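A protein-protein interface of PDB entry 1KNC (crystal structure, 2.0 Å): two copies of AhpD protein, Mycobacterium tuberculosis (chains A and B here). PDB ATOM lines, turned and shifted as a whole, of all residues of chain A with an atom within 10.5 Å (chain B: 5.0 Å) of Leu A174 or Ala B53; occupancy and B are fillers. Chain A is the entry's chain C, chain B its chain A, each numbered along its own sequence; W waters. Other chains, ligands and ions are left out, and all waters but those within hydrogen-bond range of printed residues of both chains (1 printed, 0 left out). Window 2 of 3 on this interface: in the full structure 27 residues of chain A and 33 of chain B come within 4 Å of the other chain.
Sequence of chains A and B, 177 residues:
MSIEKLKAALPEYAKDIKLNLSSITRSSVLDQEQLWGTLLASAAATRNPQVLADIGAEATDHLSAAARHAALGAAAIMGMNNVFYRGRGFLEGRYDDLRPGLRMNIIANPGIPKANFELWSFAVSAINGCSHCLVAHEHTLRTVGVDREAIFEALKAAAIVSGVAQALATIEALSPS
O of Gly B56 lies within hydrogen-bond range of NH1 of Arg B68 (3.2 Å).
OG1 of Thr A170 sits at hydrogen-bond distance from O of Gln A166, 3.0 Å away.
Among the printed residues, merely in contact across the chains: Tyr A13 with Leu B72, Thr A170 with Leu B52, Thr A170 with Leu B72, Ala A173 with Pro B49, Ala A173 with Leu B52, Leu A174 with Leu B52, Leu A174 with Ala B53 and Leu A174 with Arg B68.
Of the printed residues of chain B, Ala A173 touches Pro B49 and Leu B52.
Of chain B, only Leu B52 (3.8 Å), Ala B53 (3.8 Å) and Arg B68 (3.6 Å) come within 4 Å of Leu A174.
Ser A175 touches none of the printed residues of chain B.
Of the printed residues of chain A, Pro B49 touches Ala A173 (3.6 Å).
Of the printed residues of chain A, Ala B53 touches Leu A174.
Asp B54 touches none of the printed residues of chain A.
Of the printed residues of chain A, Leu B72 touches Tyr A13 (3.6 Å) and Thr A170 (3.7 Å).
The nearest residue of chain B that does not touch Leu A174 is Leu B72 (4.1 Å).
The nearest printed residue of chain A that does not touch Ala B53 is Ala A173 (4.01 Å).
The nearest printed residue of chain A that does not touch Arg B68 is Tyr A13 (5.8 Å).
No position is printed for both chains.
Water W1 bridges OG1 of Thr A170 (2.5 Å) and O of Leu B72 (3.1 Å).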
ATOM      1  N   PRO A  11      23.046  12.704  30.614  1.00  0.00           N
ATOM      2  CA  PRO A  11      23.669  13.310  31.790  1.00  0.00           C
ATOM      3  C   PRO A  11      22.928  12.914  33.065  1.00  0.00           C
ATOM      4  O   PRO A  11      21.768  12.508  33.018  1.00  0.00           O
ATOM      5  CB  PRO A  11      23.575  14.806  31.495  1.00  0.00           C
ATOM      6  CG  PRO A  11      22.327  14.910  30.686  1.00  0.00           C
ATOM      7  CD  PRO A  11      22.462  13.737  29.741  1.00  0.00           C
ATOM      8  N   TYR A  13      21.825  14.807  35.558  1.00  0.00           N
ATOM      9  CA  TYR A  13      20.709  15.683  35.885  1.00  0.00           C
ATOM     10  C   TYR A  13      19.503  15.414  34.982  1.00  0.00           C
ATOM     11  O   TYR A  13      18.451  16.031  35.134  1.00  0.00           O
ATOM     12  CB  TYR A  13      21.154  17.149  35.798  1.00  0.00           C
ATOM     13  CG  TYR A  13      21.892  17.507  34.529  1.00  0.00           C
ATOM     14  CD1 TYR A  13      21.216  17.610  33.310  1.00  0.00           C
ATOM     15  CD2 TYR A  13      23.270  17.734  34.542  1.00  0.00           C
ATOM     16  CE1 TYR A  13      21.892  17.929  32.136  1.00  0.00           C
ATOM     17  CE2 TYR A  13      23.955  18.053  33.373  1.00  0.00           C
ATOM     18  CZ  TYR A  13      23.257  18.149  32.173  1.00  0.00           C
ATOM     19  OH  TYR A  13      23.918  18.458  31.009  1.00  0.00           O
ATOM     20  N   GLN A 166      17.109  16.902  23.698  1.00  0.00           N
ATOM     21  CA  GLN A 166      17.540  18.105  24.398  1.00  0.00           C
ATOM     22  C   GLN A 166      18.670  17.780  25.367  1.00  0.00           C
ATOM     23  O   GLN A 166      19.683  18.479  25.410  1.00  0.00           O
ATOM     24  CB  GLN A 166      16.379  18.733  25.176  1.00  0.00           C
ATOM     25  CG  GLN A 166      16.806  19.837  26.147  1.00  0.00           C
ATOM     26  CD  GLN A 166      17.278  21.104  25.446  1.00  0.00           C
ATOM     27  OE1 GLN A 166      16.476  21.881  24.926  1.00  0.00           O
ATOM     28  NE2 GLN A 166      18.585  21.314  25.433  1.00  0.00           N
ATOM     29  N   ALA A 167      18.493  16.722  26.152  1.00  0.00           N
ATOM     30  CA  ALA A 167      19.519  16.334  27.115  1.00  0.00           C
ATOM     31  C   ALA A 167      20.844  16.013  26.427  1.00  0.00           C
ATOM     32  O   ALA A 167      21.899  16.426  26.897  1.00  0.00           O
ATOM     33  CB  ALA A 167      19.048  15.137  27.932  1.00  0.00           C
ATOM     34  N   LEU A 168      20.790  15.283  25.317  1.00  0.00           N
ATOM     35  CA  LEU A 168      22.006  14.930  24.595  1.00  0.00           C
ATOM     36  C   LEU A 168      22.683  16.113  23.919  1.00  0.00           C
ATOM     37  O   LEU A 168      23.891  16.293  24.045  1.00  0.00           O
ATOM     38  CB  LEU A 168      21.717  13.862  23.546  1.00  0.00           C
ATOM     39  CG  LEU A 168      21.543  12.436  24.064  1.00  0.00           C
ATOM     40  CD1 LEU A 168      21.253  11.516  22.885  1.00  0.00           C
ATOM     41  CD2 LEU A 168      22.816  11.990  24.787  1.00  0.00           C
ATOM     42  N   ALA A 169      21.908  16.913  23.194  1.00  0.00           N
ATOM     43  CA  ALA A 169      22.461  18.066  22.491  1.00  0.00           C
ATOM     44  C   ALA A 169      23.246  18.959  23.441  1.00  0.00           C
ATOM     45  O   ALA A 169      24.223  19.596  23.049  1.00  0.00           O
ATOM     46  CB  ALA A 169      21.345  18.862  21.826  1.00  0.00           C
ATOM     47  N   THR A 170      22.815  18.997  24.692  1.00  0.00           N
ATOM     48  CA  THR A 170      23.469  19.817  25.698  1.00  0.00           C
ATOM     49  C   THR A 170      24.883  19.357  26.037  1.00  0.00           C
ATOM     50  O   THR A 170      25.854  20.079  25.801  1.00  0.00           O
ATOM     51  CB  THR A 170      22.631  19.854  26.978  1.00  0.00           C
ATOM     52  OG1 THR A 170      21.391  20.512  26.705  1.00  0.00           O
ATOM     53  CG2 THR A 170      23.364  20.596  28.081  1.00  0.00           C
ATOM     54  N   ILE A 171      24.999  18.159  26.593  1.00  0.00           N
ATOM     55  CA  ILE A 171      26.303  17.625  26.964  1.00  0.00           C
ATOM     56  C   ILE A 171      27.227  17.512  25.757  1.00  0.00           C
ATOM     57  O   ILE A 171      28.429  17.749  25.861  1.00  0.00           O
ATOM     58  CB  ILE A 171      26.159  16.247  27.627  1.00  0.00           C
ATOM     59  CG1 ILE A 171      25.430  15.291  26.684  1.00  0.00           C
ATOM     60  CG2 ILE A 171      25.414  16.388  28.942  1.00  0.00           C
ATOM     61  CD1 ILE A 171      24.963  14.021  27.342  1.00  0.00           C
ATOM     62  N   GLU A 172      26.654  17.158  24.612  1.00  0.00           N
ATOM     63  CA  GLU A 172      27.420  17.014  23.379  1.00  0.00           C
ATOM     64  C   GLU A 172      28.148  18.320  23.063  1.00  0.00           C
ATOM     65  O   GLU A 172      29.320  18.314  22.684  1.00  0.00           O
ATOM     66  CB  GLU A 172      26.477  16.649  22.228  1.00  0.00           C
ATOM     67  CG  GLU A 172      27.171  16.316  20.914  1.00  0.00           C
ATOM     68  CD  GLU A 172      28.004  15.045  20.995  1.00  0.00           C
ATOM     69  OE1 GLU A 172      27.423  13.966  21.253  1.00  0.00           O
ATOM     70  OE2 GLU A 172      29.237  15.127  20.803  1.00  0.00           O
ATOM     71  N   ALA A 173      27.444  19.437  23.232  1.00  0.00           N
ATOM     72  CA  ALA A 173      28.000  20.758  22.962  1.00  0.00           C
ATOM     73  C   ALA A 173      28.946  21.227  24.064  1.00  0.00           C
ATOM     74  O   ALA A 173      29.804  22.081  23.836  1.00  0.00           O
ATOM     75  CB  ALA A 173      26.870  21.767  22.785  1.00  0.00           C
ATOM     76  N   LEU A 174      28.784  20.665  25.257  1.00  0.00           N
ATOM     77  CA  LEU A 174      29.622  21.029  26.394  1.00  0.00           C
ATOM     78  C   LEU A 174      30.643  19.944  26.736  1.00  0.00           C
ATOM     79  O   LEU A 174      31.071  19.825  27.884  1.00  0.00           O
ATOM     80  CB  LEU A 174      28.747  21.319  27.621  1.00  0.00           C
ATOM     81  CG  LEU A 174      27.812  22.528  27.535  1.00  0.00           C
ATOM     82  CD1 LEU A 174      26.954  22.599  28.784  1.00  0.00           C
ATOM     83  CD2 LEU A 174      28.630  23.804  27.371  1.00  0.00           C
ATOM     84  N   SER A 175      31.033  19.157  25.737  1.00  0.00           N
ATOM     85  CA  SER A 175      32.003  18.089  25.944  1.00  0.00           C
ATOM     86  C   SER A 175      33.425  18.591  25.694  1.00  0.00           C
ATOM     87  O   SER A 175      34.131  18.828  26.698  1.00  0.00           O
ATOM     88  CB  SER A 175      31.707  16.914  25.010  1.00  0.00           C
ATOM     89  OG  SER A 175      31.899  17.277  23.653  1.00  0.00           O
ATOM     90  N   PRO B  49      24.848  24.675  19.641  1.00  0.00           N
ATOM     91  CA  PRO B  49      26.040  24.278  20.397  1.00  0.00           C
ATOM     92  C   PRO B  49      27.010  25.414  20.720  1.00  0.00           C
ATOM     93  O   PRO B  49      27.438  25.566  21.865  1.00  0.00           O
ATOM     94  CB  PRO B  49      26.662  23.195  19.518  1.00  0.00           C
ATOM     95  CG  PRO B  49      26.288  23.624  18.139  1.00  0.00           C
ATOM     96  CD  PRO B  49      24.855  24.088  18.288  1.00  0.00           C
ATOM     97  N   GLN B  50      27.337  26.221  19.720  1.00  0.00           N
ATOM     98  CA  GLN B  50      28.264  27.330  19.912  1.00  0.00           C
ATOM     99  C   GLN B  50      27.840  28.275  21.034  1.00  0.00           C
ATOM    100  O   GLN B  50      28.637  28.616  21.905  1.00  0.00           O
ATOM    101  CB  GLN B  50      28.400  28.120  18.611  1.00  0.00           C
ATOM    102  CG  GLN B  50      29.571  29.079  18.604  1.00  0.00           C
ATOM    103  CD  GLN B  50      30.896  28.354  18.770  1.00  0.00           C
ATOM    104  OE1 GLN B  50      31.264  27.946  19.881  1.00  0.00           O
ATOM    105  NE2 GLN B  50      31.612  28.170  17.659  1.00  0.00           N
ATOM    106  N   VAL B  51      26.584  28.705  21.001  1.00  0.00           N
ATOM    107  CA  VAL B  51      26.076  29.619  22.014  1.00  0.00           C
ATOM    108  C   VAL B  51      26.139  28.981  23.400  1.00  0.00           C
ATOM    109  O   VAL B  51      26.612  29.596  24.355  1.00  0.00           O
ATOM    110  CB  VAL B  51      24.629  30.042  21.693  1.00  0.00           C
ATOM    111  CG1 VAL B  51      24.109  30.999  22.756  1.00  0.00           C
ATOM    112  CG2 VAL B  51      24.587  30.702  20.327  1.00  0.00           C
ATOM    113  N   LEU B  52      25.679  27.740  23.502  1.00  0.00           N
ATOM    114  CA  LEU B  52      25.703  27.032  24.769  1.00  0.00           C
ATOM    115  C   LEU B  52      27.138  26.962  25.288  1.00  0.00           C
ATOM    116  O   LEU B  52      27.397  27.240  26.458  1.00  0.00           O
ATOM    117  CB  LEU B  52      25.135  25.624  24.596  1.00  0.00           C
ATOM    118  CG  LEU B  52      25.233  24.685  25.800  1.00  0.00           C
ATOM    119  CD1 LEU B  52      24.602  25.327  27.035  1.00  0.00           C
ATOM    120  CD2 LEU B  52      24.537  23.380  25.460  1.00  0.00           C
ATOM    121  N   ALA B  53      28.071  26.595  24.414  1.00  0.00           N
ATOM    122  CA  ALA B  53      29.469  26.505  24.817  1.00  0.00           C
ATOM    123  C   ALA B  53      29.986  27.836  25.375  1.00  0.00           C
ATOM    124  O   ALA B  53      30.585  27.859  26.449  1.00  0.00           O
ATOM    125  CB  ALA B  53      30.328  26.051  23.639  1.00  0.00           C
ATOM    126  N   ASP B  54      29.755  28.939  24.661  1.00  0.00           N
ATOM    127  CA  ASP B  54      30.222  30.251  25.124  1.00  0.00           C
ATOM    128  C   ASP B  54      29.578  30.687  26.442  1.00  0.00           C
ATOM    129  O   ASP B  54      30.272  31.121  27.367  1.00  0.00           O
ATOM    130  CB  ASP B  54      29.972  31.334  24.066  1.00  0.00           C
ATOM    131  CG  ASP B  54      30.775  31.110  22.784  1.00  0.00           C
ATOM    132  OD1 ASP B  54      31.793  30.392  22.820  1.00  0.00           O
ATOM    133  OD2 ASP B  54      30.393  31.672  21.740  1.00  0.00           O
ATOM    134  N   ILE B  55      28.254  30.585  26.524  1.00  0.00           N
ATOM    135  CA  ILE B  55      27.531  30.967  27.734  1.00  0.00           C
ATOM    136  C   ILE B  55      27.976  30.089  28.900  1.00  0.00           C
ATOM    137  O   ILE B  55      28.229  30.586  29.995  1.00  0.00           O
ATOM    138  CB  ILE B  55      25.997  30.817  27.543  1.00  0.00           C
ATOM    139  CG1 ILE B  55      25.490  31.846  26.527  1.00  0.00           C
ATOM    140  CG2 ILE B  55      25.275  30.975  28.877  1.00  0.00           C
ATOM    141  CD1 ILE B  55      25.677  33.284  26.946  1.00  0.00           C
ATOM    142  N   GLY B  56      28.068  28.785  28.651  1.00  0.00           N
ATOM    143  CA  GLY B  56      28.475  27.854  29.689  1.00  0.00           C
ATOM    144  C   GLY B  56      29.868  28.125  30.218  1.00  0.00           C
ATOM    145  O   GLY B  56      30.166  27.847  31.382  1.00  0.00           O
ATOM    146  N   ALA B  57      30.723  28.670  29.359  1.00  0.00           N
ATOM    147  CA  ALA B  57      32.095  28.989  29.728  1.00  0.00           C
ATOM    148  C   ALA B  57      32.144  30.149  30.714  1.00  0.00           C
ATOM    149  O   ALA B  57      32.885  30.106  31.695  1.00  0.00           O
ATOM    150  CB  ALA B  57      32.906  29.329  28.482  1.00  0.00           C
ATOM    151  N   ARG B  68      24.265  25.141  38.184  1.00  0.00           N
ATOM    152  CA  ARG B  68      24.563  24.789  36.799  1.00  0.00           C
ATOM    153  C   ARG B  68      23.831  23.503  36.414  1.00  0.00           C
ATOM    154  O   ARG B  68      23.196  23.426  35.357  1.00  0.00           O
ATOM    155  CB  ARG B  68      26.074  24.605  36.616  1.00  0.00           C
ATOM    156  CG  ARG B  68      26.506  24.212  35.207  1.00  0.00           C
ATOM    157  CD  ARG B  68      27.996  23.859  35.143  1.00  0.00           C
ATOM    158  NE  ARG B  68      28.385  23.389  33.813  1.00  0.00           N
ATOM    159  CZ  ARG B  68      28.670  24.186  32.787  1.00  0.00           C
ATOM    160  NH1 ARG B  68      28.623  25.504  32.928  1.00  0.00           N
ATOM    161  NH2 ARG B  68      28.980  23.664  31.608  1.00  0.00           N
ATOM    162  N   LEU B  72      20.676  23.191  33.559  1.00  0.00           N
ATOM    163  CA  LEU B  72      20.736  22.303  32.406  1.00  0.00           C
ATOM    164  C   LEU B  72      19.641  21.251  32.572  1.00  0.00           C
ATOM    165  O   LEU B  72      19.030  20.818  31.596  1.00  0.00           O
ATOM    166  CB  LEU B  72      22.122  21.647  32.290  1.00  0.00           C
ATOM    167  CG  LEU B  72      23.295  22.604  31.987  1.00  0.00           C
ATOM    168  CD1 LEU B  72      24.616  21.833  32.047  1.00  0.00           C
ATOM    169  CD2 LEU B  72      23.123  23.245  30.600  1.00  0.00           C
HETATM  170  O   HOH W   1      19.977  19.995  28.724  1.00  0.00           O
